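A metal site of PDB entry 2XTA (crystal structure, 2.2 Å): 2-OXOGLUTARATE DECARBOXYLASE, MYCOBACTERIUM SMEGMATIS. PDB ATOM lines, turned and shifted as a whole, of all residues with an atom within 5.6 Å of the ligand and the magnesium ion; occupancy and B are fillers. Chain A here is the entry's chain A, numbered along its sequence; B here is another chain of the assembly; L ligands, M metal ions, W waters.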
ATOM      1  N   HIS A 180      -4.300  25.912  13.186  1.00  0.00           N
ATOM      2  CA  HIS A 180      -5.336  26.773  13.773  1.00  0.00           C
ATOM      3  C   HIS A 180      -5.172  28.315  13.585  1.00  0.00           C
ATOM      4  O   HIS A 180      -6.189  29.033  13.671  1.00  0.00           O
ATOM      5  CB  HIS A 180      -5.499  26.479  15.266  1.00  0.00           C
ATOM      6  CG  HIS A 180      -4.281  26.798  16.088  1.00  0.00           C
ATOM      7  ND1 HIS A 180      -4.011  28.086  16.494  1.00  0.00           N
ATOM      8  CD2 HIS A 180      -3.295  25.982  16.509  1.00  0.00           C
ATOM      9  CE1 HIS A 180      -2.857  28.015  17.155  1.00  0.00           C
ATOM     10  NE2 HIS A 180      -2.401  26.767  17.201  1.00  0.00           N
ATOM     11  N   ARG A 181      -3.937  28.844  13.370  1.00  0.00           N
ATOM     12  CA  ARG A 181      -3.723  30.297  13.245  1.00  0.00           C
ATOM     13  C   ARG A 181      -4.503  30.905  12.049  1.00  0.00           C
ATOM     14  O   ARG A 181      -4.262  30.560  10.904  1.00  0.00           O
ATOM     15  CB  ARG A 181      -2.228  30.654  13.153  1.00  0.00           C
ATOM     16  CG  ARG A 181      -1.964  32.164  13.221  1.00  0.00           C
ATOM     17  CD  ARG A 181      -0.491  32.540  13.221  1.00  0.00           C
ATOM     18  NE  ARG A 181       0.302  31.848  14.269  1.00  0.00           N
ATOM     19  CZ  ARG A 181       0.283  32.183  15.556  1.00  0.00           C
ATOM     20  NH1 ARG A 181      -0.488  33.173  15.979  1.00  0.00           N
ATOM     21  NH2 ARG A 181       1.034  31.527  16.422  1.00  0.00           N
ATOM     22  N   SER A 245      -4.565  18.917  16.645  1.00  0.00           N
ATOM     23  CA  SER A 245      -3.594  19.940  17.008  1.00  0.00           C
ATOM     24  C   SER A 245      -2.187  19.532  16.497  1.00  0.00           C
ATOM     25  O   SER A 245      -1.318  20.384  16.409  1.00  0.00           O
ATOM     26  CB  SER A 245      -3.566  20.131  18.513  1.00  0.00           C
ATOM     27  OG  SER A 245      -4.805  20.646  18.985  1.00  0.00           O
ATOM     28  N   HIS A 246      -1.979  18.234  16.148  1.00  0.00           N
ATOM     29  CA  HIS A 246      -0.711  17.695  15.614  1.00  0.00           C
ATOM     30  C   HIS A 246      -0.436  18.346  14.293  1.00  0.00           C
ATOM     31  O   HIS A 246      -1.143  18.095  13.314  1.00  0.00           O
ATOM     32  CB  HIS A 246      -0.771  16.156  15.467  1.00  0.00           C
ATOM     33  CG  HIS A 246      -0.854  15.430  16.774  1.00  0.00           C
ATOM     34  ND1 HIS A 246      -1.847  15.707  17.704  1.00  0.00           N
ATOM     35  CD2 HIS A 246      -0.043  14.455  17.256  1.00  0.00           C
ATOM     36  CE1 HIS A 246      -1.606  14.906  18.734  1.00  0.00           C
ATOM     37  NE2 HIS A 246      -0.556  14.117  18.509  1.00  0.00           N
ATOM     38  N   LEU A 247       0.518  19.281  14.299  1.00  0.00           N
ATOM     39  CA  LEU A 247       0.889  20.086  13.155  1.00  0.00           C
ATOM     40  C   LEU A 247       1.409  19.210  12.014  1.00  0.00           C
ATOM     41  O   LEU A 247       2.187  18.299  12.254  1.00  0.00           O
ATOM     42  CB  LEU A 247       1.950  21.148  13.550  1.00  0.00           C
ATOM     43  CG  LEU A 247       1.534  22.188  14.614  1.00  0.00           C
ATOM     44  CD1 LEU A 247       2.688  23.028  15.030  1.00  0.00           C
ATOM     45  CD2 LEU A 247       0.391  23.084  14.121  1.00  0.00           C
ATOM     46  N   GLY A 285       3.019  26.469   8.989  1.00  0.00           N
ATOM     47  CA  GLY A 285       3.819  27.349   9.834  1.00  0.00           C
ATOM     48  C   GLY A 285       5.282  27.019   9.525  1.00  0.00           C
ATOM     49  O   GLY A 285       5.574  25.895   9.077  1.00  0.00           O
ATOM     50  N   ASP A 286       6.204  27.973   9.786  1.00  0.00           N
ATOM     51  CA  ASP A 286       7.602  27.832   9.426  1.00  0.00           C
ATOM     52  C   ASP A 286       8.359  26.792  10.262  1.00  0.00           C
ATOM     53  O   ASP A 286       9.183  26.085   9.692  1.00  0.00           O
ATOM     54  CB  ASP A 286       8.349  29.201   9.490  1.00  0.00           C
ATOM     55  CG  ASP A 286       8.302  29.929  10.822  1.00  0.00           C
ATOM     56  OD1 ASP A 286       7.171  30.233  11.303  1.00  0.00           O
ATOM     57  OD2 ASP A 286       9.373  30.243  11.351  1.00  0.00           O
ATOM     58  N   ALA A 287       8.184  26.762  11.575  1.00  0.00           N
ATOM     59  CA  ALA A 287       8.903  25.793  12.417  1.00  0.00           C
ATOM     60  C   ALA A 287       8.401  24.347  12.121  1.00  0.00           C
ATOM     61  O   ALA A 287       9.230  23.457  11.960  1.00  0.00           O
ATOM     62  CB  ALA A 287       8.746  26.134  13.901  1.00  0.00           C
ATOM     63  N   ALA A 288       7.095  24.151  11.952  1.00  0.00           N
ATOM     64  CA  ALA A 288       6.486  22.841  11.667  1.00  0.00           C
ATOM     65  C   ALA A 288       6.827  22.300  10.262  1.00  0.00           C
ATOM     66  O   ALA A 288       7.023  21.104  10.108  1.00  0.00           O
ATOM     67  CB  ALA A 288       4.990  22.915  11.849  1.00  0.00           C
ATOM     68  N   PHE A 289       6.903  23.187   9.229  1.00  0.00           N
ATOM     69  CA  PHE A 289       7.211  22.795   7.847  1.00  0.00           C
ATOM     70  C   PHE A 289       8.623  22.236   7.752  1.00  0.00           C
ATOM     71  O   PHE A 289       8.878  21.328   6.962  1.00  0.00           O
ATOM     72  CB  PHE A 289       7.030  23.988   6.860  1.00  0.00           C
ATOM     73  CG  PHE A 289       6.922  23.583   5.406  1.00  0.00           C
ATOM     74  CD1 PHE A 289       5.801  22.923   4.916  1.00  0.00           C
ATOM     75  CD2 PHE A 289       7.955  23.855   4.515  1.00  0.00           C
ATOM     76  CE1 PHE A 289       5.702  22.555   3.576  1.00  0.00           C
ATOM     77  CE2 PHE A 289       7.867  23.483   3.167  1.00  0.00           C
ATOM     78  CZ  PHE A 289       6.740  22.827   2.707  1.00  0.00           C
ATOM     79  N   GLN A 292       8.768  18.619  10.739  1.00  0.00           N
ATOM     80  CA  GLN A 292       7.905  17.418  10.708  1.00  0.00           C
ATOM     81  C   GLN A 292       8.202  16.568   9.494  1.00  0.00           C
ATOM     82  O   GLN A 292       8.082  17.046   8.369  1.00  0.00           O
ATOM     83  CB  GLN A 292       6.419  17.806  10.753  1.00  0.00           C
ATOM     84  CG  GLN A 292       5.984  18.344  12.124  1.00  0.00           C
ATOM     85  CD  GLN A 292       5.928  17.259  13.186  1.00  0.00           C
ATOM     86  OE1 GLN A 292       5.225  16.254  13.034  1.00  0.00           O
ATOM     87  NE2 GLN A 292       6.637  17.459  14.282  1.00  0.00           N
ATOM     88  N   VAL A 317       3.103  30.319   6.335  1.00  0.00           N
ATOM     89  CA  VAL A 317       2.944  31.550   7.101  1.00  0.00           C
ATOM     90  C   VAL A 317       4.206  31.633   7.945  1.00  0.00           C
ATOM     91  O   VAL A 317       4.286  31.075   9.043  1.00  0.00           O
ATOM     92  CB  VAL A 317       1.625  31.569   7.921  1.00  0.00           C
ATOM     93  CG1 VAL A 317       1.486  32.868   8.704  1.00  0.00           C
ATOM     94  CG2 VAL A 317       0.413  31.350   7.005  1.00  0.00           C
ATOM     95  N   ASN A 318       5.247  32.239   7.368  1.00  0.00           N
ATOM     96  CA  ASN A 318       6.573  32.334   7.959  1.00  0.00           C
ATOM     97  C   ASN A 318       6.728  33.566   8.812  1.00  0.00           C
ATOM     98  O   ASN A 318       7.245  34.582   8.354  1.00  0.00           O
ATOM     99  CB  ASN A 318       7.635  32.287   6.857  1.00  0.00           C
ATOM    100  CG  ASN A 318       9.058  32.195   7.342  1.00  0.00           C
ATOM    101  OD1 ASN A 318       9.354  32.160   8.535  1.00  0.00           O
ATOM    102  ND2 ASN A 318       9.973  32.135   6.405  1.00  0.00           N
ATOM    103  N   ASN A 319       6.325  33.459  10.095  1.00  0.00           N
ATOM    104  CA  ASN A 319       6.390  34.567  11.064  1.00  0.00           C
ATOM    105  C   ASN A 319       7.713  34.542  11.834  1.00  0.00           C
ATOM    106  O   ASN A 319       7.879  35.250  12.834  1.00  0.00           O
ATOM    107  CB  ASN A 319       5.196  34.559  12.010  1.00  0.00           C
ATOM    108  CG  ASN A 319       4.923  33.258  12.718  1.00  0.00           C
ATOM    109  OD1 ASN A 319       5.789  32.364  12.783  1.00  0.00           O
ATOM    110  ND2 ASN A 319       3.711  33.147  13.274  1.00  0.00           N
ATOM    111  N   GLN A 320       8.667  33.711  11.336  1.00  0.00           N
ATOM    112  CA  GLN A 320      10.068  33.610  11.752  1.00  0.00           C
ATOM    113  C   GLN A 320      10.226  33.345  13.256  1.00  0.00           C
ATOM    114  O   GLN A 320      11.090  33.923  13.933  1.00  0.00           O
ATOM    115  CB  GLN A 320      10.812  34.915  11.356  1.00  0.00           C
ATOM    116  CG  GLN A 320      10.571  35.347   9.881  1.00  0.00           C
ATOM    117  CD  GLN A 320      11.072  36.759   9.635  1.00  0.00           C
ATOM    118  OE1 GLN A 320      12.175  37.123  10.044  1.00  0.00           O
ATOM    119  NE2 GLN A 320      10.268  37.608   8.995  1.00  0.00           N
ATOM    120  N   ILE A 321       9.353  32.452  13.775  1.00  0.00           N
ATOM    121  CA  ILE A 321       9.251  32.072  15.183  1.00  0.00           C
ATOM    122  C   ILE A 321       8.327  30.875  15.288  1.00  0.00           C
ATOM    123  O   ILE A 321       7.411  30.687  14.482  1.00  0.00           O
ATOM    124  CB  ILE A 321       8.786  33.274  16.113  1.00  0.00           C
ATOM    125  CG1 ILE A 321       9.137  33.036  17.598  1.00  0.00           C
ATOM    126  CG2 ILE A 321       7.308  33.768  15.872  1.00  0.00           C
ATOM    127  CD1 ILE A 321       9.112  34.271  18.431  1.00  0.00           C
ATOM    128  N   GLY A 322       8.632  30.052  16.266  1.00  0.00           N
ATOM    129  CA  GLY A 322       7.866  28.848  16.593  1.00  0.00           C
ATOM    130  C   GLY A 322       7.718  28.848  18.094  1.00  0.00           C
ATOM    131  O   GLY A 322       8.640  28.421  18.793  1.00  0.00           O
ATOM    132  N   PHE A 323       6.614  29.453  18.594  1.00  0.00           N
ATOM    133  CA  PHE A 323       6.338  29.626  20.025  1.00  0.00           C
ATOM    134  C   PHE A 323       7.412  30.555  20.646  1.00  0.00           C
ATOM    135  O   PHE A 323       7.300  31.755  20.474  1.00  0.00           O
ATOM    136  CB  PHE A 323       6.208  28.263  20.772  1.00  0.00           C
ATOM    137  CG  PHE A 323       5.453  28.259  22.093  1.00  0.00           C
ATOM    138  CD1 PHE A 323       5.428  29.392  22.894  1.00  0.00           C
ATOM    139  CD2 PHE A 323       4.814  27.111  22.554  1.00  0.00           C
ATOM    140  CE1 PHE A 323       4.738  29.396  24.118  1.00  0.00           C
ATOM    141  CE2 PHE A 323       4.148  27.109  23.776  1.00  0.00           C
ATOM    142  CZ  PHE A 323       4.109  28.239  24.558  1.00  0.00           C
ATOM    143  N   ARG A 384       4.453  37.631  14.047  1.00  0.00           N
ATOM    144  CA  ARG A 384       3.379  37.283  14.963  1.00  0.00           C
ATOM    145  C   ARG A 384       3.291  38.413  15.985  1.00  0.00           C
ATOM    146  O   ARG A 384       4.188  38.548  16.807  1.00  0.00           O
ATOM    147  CB  ARG A 384       3.703  35.899  15.589  1.00  0.00           C
ATOM    148  CG  ARG A 384       2.593  35.273  16.428  1.00  0.00           C
ATOM    149  CD  ARG A 384       3.206  34.214  17.327  1.00  0.00           C
ATOM    150  NE  ARG A 384       3.905  34.834  18.451  1.00  0.00           N
ATOM    151  CZ  ARG A 384       4.897  34.277  19.134  1.00  0.00           C
ATOM    152  NH1 ARG A 384       5.337  33.076  18.824  1.00  0.00           N
ATOM    153  NH2 ARG A 384       5.484  34.944  20.124  1.00  0.00           N
ATOM    154  N   HIS A 388       2.536  33.866  21.858  1.00  0.00           N
ATOM    155  CA  HIS A 388       2.000  32.629  21.325  1.00  0.00           C
ATOM    156  C   HIS A 388       0.620  32.301  21.920  1.00  0.00           C
ATOM    157  O   HIS A 388      -0.248  31.810  21.183  1.00  0.00           O
ATOM    158  CB  HIS A 388       2.984  31.506  21.616  1.00  0.00           C
ATOM    159  CG  HIS A 388       2.660  30.242  20.892  1.00  0.00           C
ATOM    160  ND1 HIS A 388       2.908  30.122  19.539  1.00  0.00           N
ATOM    161  CD2 HIS A 388       2.116  29.105  21.356  1.00  0.00           C
ATOM    162  CE1 HIS A 388       2.523  28.899  19.229  1.00  0.00           C
ATOM    163  NE2 HIS A 388       2.034  28.259  20.282  1.00  0.00           N
ATOM    164  N   GLN B 542      10.593  20.905  23.036  1.00  0.00           N
ATOM    165  CA  GLN B 542      10.040  22.112  22.399  1.00  0.00           C
ATOM    166  C   GLN B 542       9.803  23.209  23.430  1.00  0.00           C
ATOM    167  O   GLN B 542       9.076  22.980  24.396  1.00  0.00           O
ATOM    168  CB  GLN B 542       8.749  21.791  21.644  1.00  0.00           C
ATOM    169  CG  GLN B 542       9.009  21.102  20.303  1.00  0.00           C
ATOM    170  CD  GLN B 542       7.881  20.186  19.920  1.00  0.00           C
ATOM    171  OE1 GLN B 542       6.757  20.310  20.397  1.00  0.00           O
ATOM    172  NE2 GLN B 542       8.176  19.225  19.059  1.00  0.00           N
ATOM    173  N   ASP B 543      10.511  24.346  23.274  1.00  0.00           N
ATOM    174  CA  ASP B 543      10.430  25.508  24.177  1.00  0.00           C
ATOM    175  C   ASP B 543      10.801  25.179  25.640  1.00  0.00           C
ATOM    176  O   ASP B 543      10.334  25.841  26.569  1.00  0.00           O
ATOM    177  CB  ASP B 543       9.024  26.148  24.095  1.00  0.00           C
ATOM    178  CG  ASP B 543       8.638  26.445  22.656  1.00  0.00           C
ATOM    179  OD1 ASP B 543       9.222  27.391  22.071  1.00  0.00           O
ATOM    180  OD2 ASP B 543       7.858  25.658  22.086  1.00  0.00           O
ATOM    181  N   LEU B 591      10.925  21.327  15.768  1.00  0.00           N
ATOM    182  CA  LEU B 591       9.554  20.871  15.947  1.00  0.00           C
ATOM    183  C   LEU B 591       9.437  19.423  15.436  1.00  0.00           C
ATOM    184  O   LEU B 591       8.778  19.170  14.423  1.00  0.00           O
ATOM    185  CB  LEU B 591       8.563  21.830  15.253  1.00  0.00           C
ATOM    186  CG  LEU B 591       7.209  21.997  15.925  1.00  0.00           C
ATOM    187  CD1 LEU B 591       6.515  23.221  15.431  1.00  0.00           C
ATOM    188  CD2 LEU B 591       6.293  20.738  15.738  1.00  0.00           C
ATOM    189  N   GLU B 593       9.258  15.146  16.971  1.00  0.00           N
ATOM    190  CA  GLU B 593       9.079  14.230  18.081  1.00  0.00           C
ATOM    191  C   GLU B 593       9.910  12.996  17.792  1.00  0.00           C
ATOM    192  O   GLU B 593      10.753  12.652  18.594  1.00  0.00           O
ATOM    193  CB  GLU B 593       7.590  13.889  18.338  1.00  0.00           C
ATOM    194  CG  GLU B 593       6.840  15.039  19.009  1.00  0.00           C
ATOM    195  CD  GLU B 593       6.367  16.148  18.090  1.00  0.00           C
ATOM    196  OE1 GLU B 593       6.253  17.299  18.550  1.00  0.00           O
ATOM    197  OE2 GLU B 593       6.110  15.870  16.903  1.00  0.00           O
ATOM    198  N   GLN B 617       5.926  18.874  24.486  1.00  0.00           N
ATOM    199  CA  GLN B 617       5.225  20.140  24.724  1.00  0.00           C
ATOM    200  C   GLN B 617       3.986  19.814  25.576  1.00  0.00           C
ATOM    201  O   GLN B 617       3.738  20.425  26.614  1.00  0.00           O
ATOM    202  CB  GLN B 617       4.886  20.836  23.387  1.00  0.00           C
ATOM    203  CG  GLN B 617       4.218  22.183  23.570  1.00  0.00           C
ATOM    204  CD  GLN B 617       4.983  23.309  22.933  1.00  0.00           C
ATOM    205  OE1 GLN B 617       4.568  23.869  21.920  1.00  0.00           O
ATOM    206  NE2 GLN B 617       6.085  23.704  23.554  1.00  0.00           N
ATOM    207  N   PHE B 621       1.557  14.642  22.069  1.00  0.00           N
ATOM    208  CA  PHE B 621       2.359  14.690  20.850  1.00  0.00           C
ATOM    209  C   PHE B 621       3.451  13.644  20.807  1.00  0.00           C
ATOM    210  O   PHE B 621       4.038  13.454  19.732  1.00  0.00           O
ATOM    211  CB  PHE B 621       2.962  16.098  20.668  1.00  0.00           C
ATOM    212  CG  PHE B 621       1.915  17.182  20.578  1.00  0.00           C
ATOM    213  CD1 PHE B 621       1.876  18.206  21.520  1.00  0.00           C
ATOM    214  CD2 PHE B 621       0.962  17.170  19.566  1.00  0.00           C
ATOM    215  CE1 PHE B 621       0.884  19.196  21.464  1.00  0.00           C
ATOM    216  CE2 PHE B 621      -0.029  18.160  19.510  1.00  0.00           C
ATOM    217  CZ  PHE B 621      -0.059  19.167  20.464  1.00  0.00           C
ATOM    218  N   HIS B 661      -4.551  17.997  24.247  1.00  0.00           N
ATOM    219  CA  HIS B 661      -3.881  18.743  25.318  1.00  0.00           C
ATOM    220  C   HIS B 661      -4.343  18.175  26.643  1.00  0.00           C
ATOM    221  O   HIS B 661      -4.582  18.915  27.601  1.00  0.00           O
ATOM    222  CB  HIS B 661      -4.184  20.258  25.206  1.00  0.00           C
ATOM    223  CG  HIS B 661      -3.628  20.844  23.948  1.00  0.00           C
ATOM    224  ND1 HIS B 661      -4.383  20.898  22.803  1.00  0.00           N
ATOM    225  CD2 HIS B 661      -2.377  21.284  23.689  1.00  0.00           C
ATOM    226  CE1 HIS B 661      -3.578  21.391  21.876  1.00  0.00           C
ATOM    227  NE2 HIS B 661      -2.365  21.658  22.366  1.00  0.00           N
HETATM  228  N1  LIG L   1       4.221  18.953  17.891  1.00  0.00           N
HETATM  229  C1  LIG L   1       3.249  18.692  17.044  1.00  0.00           C
HETATM  230  C2  LIG L   1       3.383  17.532  16.084  1.00  0.00           C
HETATM  231  N2  LIG L   1       2.167  19.436  17.026  1.00  0.00           N
HETATM  232  C3  LIG L   1       2.018  20.451  17.901  1.00  0.00           C
HETATM  233  N3  LIG L   1       0.844  21.191  17.909  1.00  0.00           N
HETATM  234  C4  LIG L   1       3.031  20.774  18.801  1.00  0.00           C
HETATM  235  C5  LIG L   1       4.168  19.988  18.736  1.00  0.00           C
HETATM  236  C6  LIG L   1       2.936  21.952  19.767  1.00  0.00           C
HETATM  237  N4  LIG L   1       2.997  23.287  19.108  1.00  0.00           N
HETATM  238  C7  LIG L   1       1.924  24.001  18.972  1.00  0.00           C
HETATM  239  S1  LIG L   1       2.260  25.501  18.212  1.00  0.00           S
HETATM  240  C8  LIG L   1       3.969  25.102  18.162  1.00  0.00           C
HETATM  241  C9  LIG L   1       4.114  23.869  18.692  1.00  0.00           C
HETATM  242  C10 LIG L   1       5.492  23.259  18.753  1.00  0.00           C
HETATM  243  C11 LIG L   1       4.987  26.030  17.515  1.00  0.00           C
HETATM  244  C12 LIG L   1       4.536  26.208  16.064  1.00  0.00           C
HETATM  245  O1  LIG L   1       5.517  26.857  15.231  1.00  0.00           O
HETATM  246  P1  LIG L   1       5.127  27.298  13.740  1.00  0.00           P
HETATM  247  O2  LIG L   1       5.005  26.096  12.891  1.00  0.00           O
HETATM  248  O3  LIG L   1       6.212  28.332  13.146  1.00  0.00           O
HETATM  249  O4  LIG L   1       3.675  28.014  13.841  1.00  0.00           O
HETATM  250  P2  LIG L   1       3.175  29.339  14.367  1.00  0.00           P
HETATM  251  O5  LIG L   1       2.484  29.149  15.789  1.00  0.00           O
HETATM  252  O6  LIG L   1       4.322  30.299  14.449  1.00  0.00           O
HETATM  253  O7  LIG L   1       2.183  29.952  13.264  1.00  0.00           O
HETATM  254 MG    MG M   1       5.953  30.309  13.134  1.00  0.00          MG
HETATM  255  O   HOH W   1       2.226  25.513  12.496  1.00  0.00           O
HETATM  256  O   HOH W   2       4.769  30.883  17.087  1.00  0.00           O
HETATM  257  O   HOH W   3       0.835  28.069  11.861  1.00  0.00           O
HETATM  258  O   HOH W   4       4.565  30.190  11.460  1.00  0.00           O
HETATM  259  O   HOH W   5       3.526  14.265  17.315  1.00  0.00           O
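The nearest printed residue that does not touch the magnesium ion is Gly 322 (4.1 Å).
Water W4 lies within hydrogen-bond range of the backbone carbonyl oxygen of Val 317, an oxygen (O7) of the ligand and the backbone NH of Asp 286. Water W2 lies within hydrogen-bond range of N of Phe 323, NH1 of Arg 384, O5 of the ligand and ND1 of His 388. Water W5 bridges O of Phe 621 of chain B (2.6 Å) and OE2 of Glu 593 of chain B (3.1 Å).
The side-chain amide oxygen of Gln 617 of chain B sits close to a nitrogen (N4) of the ligand, 3.3 Å away. CA of His 246 touches N2 of the ligand, at 3.6 Å. C of Gly 285 touches O2 of the ligand, 3.5 Å away. Gln 292 touches the ligand (NE2 to C2, 3.7 Å). Gly 322 touches the ligand. N of Phe 323 touches C11 of the ligand, 3.9 Å away. OE1 of Gln 542 of chain B touches C5 of the ligand (3.1 Å). Leu 591 of chain B touches the ligand (CD1 to C10, 3.5 Å). CZ of Phe 621 of chain B touches N3 of the ligand, at 3.4 Å. Hydrophobic or aromatic side chains that line the ligand: Leu 247, Ala 287, Ala 288, His 388, Leu 591 of chain B and Phe 621 of chain B. The nearest printed residue that does not touch the ligand is Asp 543 of chain B (4.7 Å).
The magnesium ion is bound by an oxygen (O3) of the ligand. O of Ile 321 binds the magnesium ion (2.0 Å). The side-chain amide oxygen (OD1) of Asn 319 is bound to the magnesium ion (2.1 Å). O6 of the ligand is bound to the magnesium ion (2.1 Å). Water W4 binds the magnesium ion, at 2.2 Å. OD1 of Asp 286 is bound to the magnesium ion, at 2.2 Å.
The backbone carbonyl oxygen (O) of Leu 591 of chain B lies within hydrogen-bond range of the side-chain amide nitrogen (NE2) of Gln 292 (2.7 Å). O of Phe 323 sits at hydrogen-bond distance from NH1 of Arg 384 (2.9 Å). The side-chain carboxylate of Glu 593 of chain B is in hydrogen-bond range of the side-chain amide nitrogen of Gln 542 of chain B (2.8 Å). The side-chain carboxylate (OD2) of Asp 543 of chain B sits at hydrogen-bond distance from the side-chain amide nitrogen (NE2) of Gln 617 of chain B, 3.0 Å away. The side-chain amide oxygen of Asn 318 sits close to the side-chain carboxylate of Asp 286, at 3.4 Å. The backbone carbonyl oxygen of Gln 542 of chain B sits at hydrogen-bond distance from the side-chain amide nitrogen of Gln 617 of chain B. The side-chain amide nitrogen of Gln 292 is in hydrogen-bond range of the side-chain carboxylate of Glu 593 of chain B (3.1 Å).
The backbone NH of Ala 287 lies close to an oxygen (O3) of the ligand, at 3.0 Å. The side-chain carboxylate (OE1) of Glu 593 of chain B is in hydrogen-bond range of a nitrogen (N1) of the ligand, 2.7 Å away. The guanidinium group of Arg 181 is in salt-bridge range of an oxygen (O7) of the ligand (2.9 Å). A ring nitrogen (NE2) of His 388 lies close to a sulfur (S1) of the ligand, 3.5 Å away. N of Ala 288 sits at hydrogen-bond distance from O2 of the ligand (3.0 Å). N3 of the ligand is in hydrogen-bond range of O of Ser 245 (2.8 Å). The backbone NH of Asp 286 lies close to an oxygen (O3) of the ligand (3.4 Å). N of Leu 247 lies within hydrogen-bond range of N2 of the ligand (3.2 Å).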
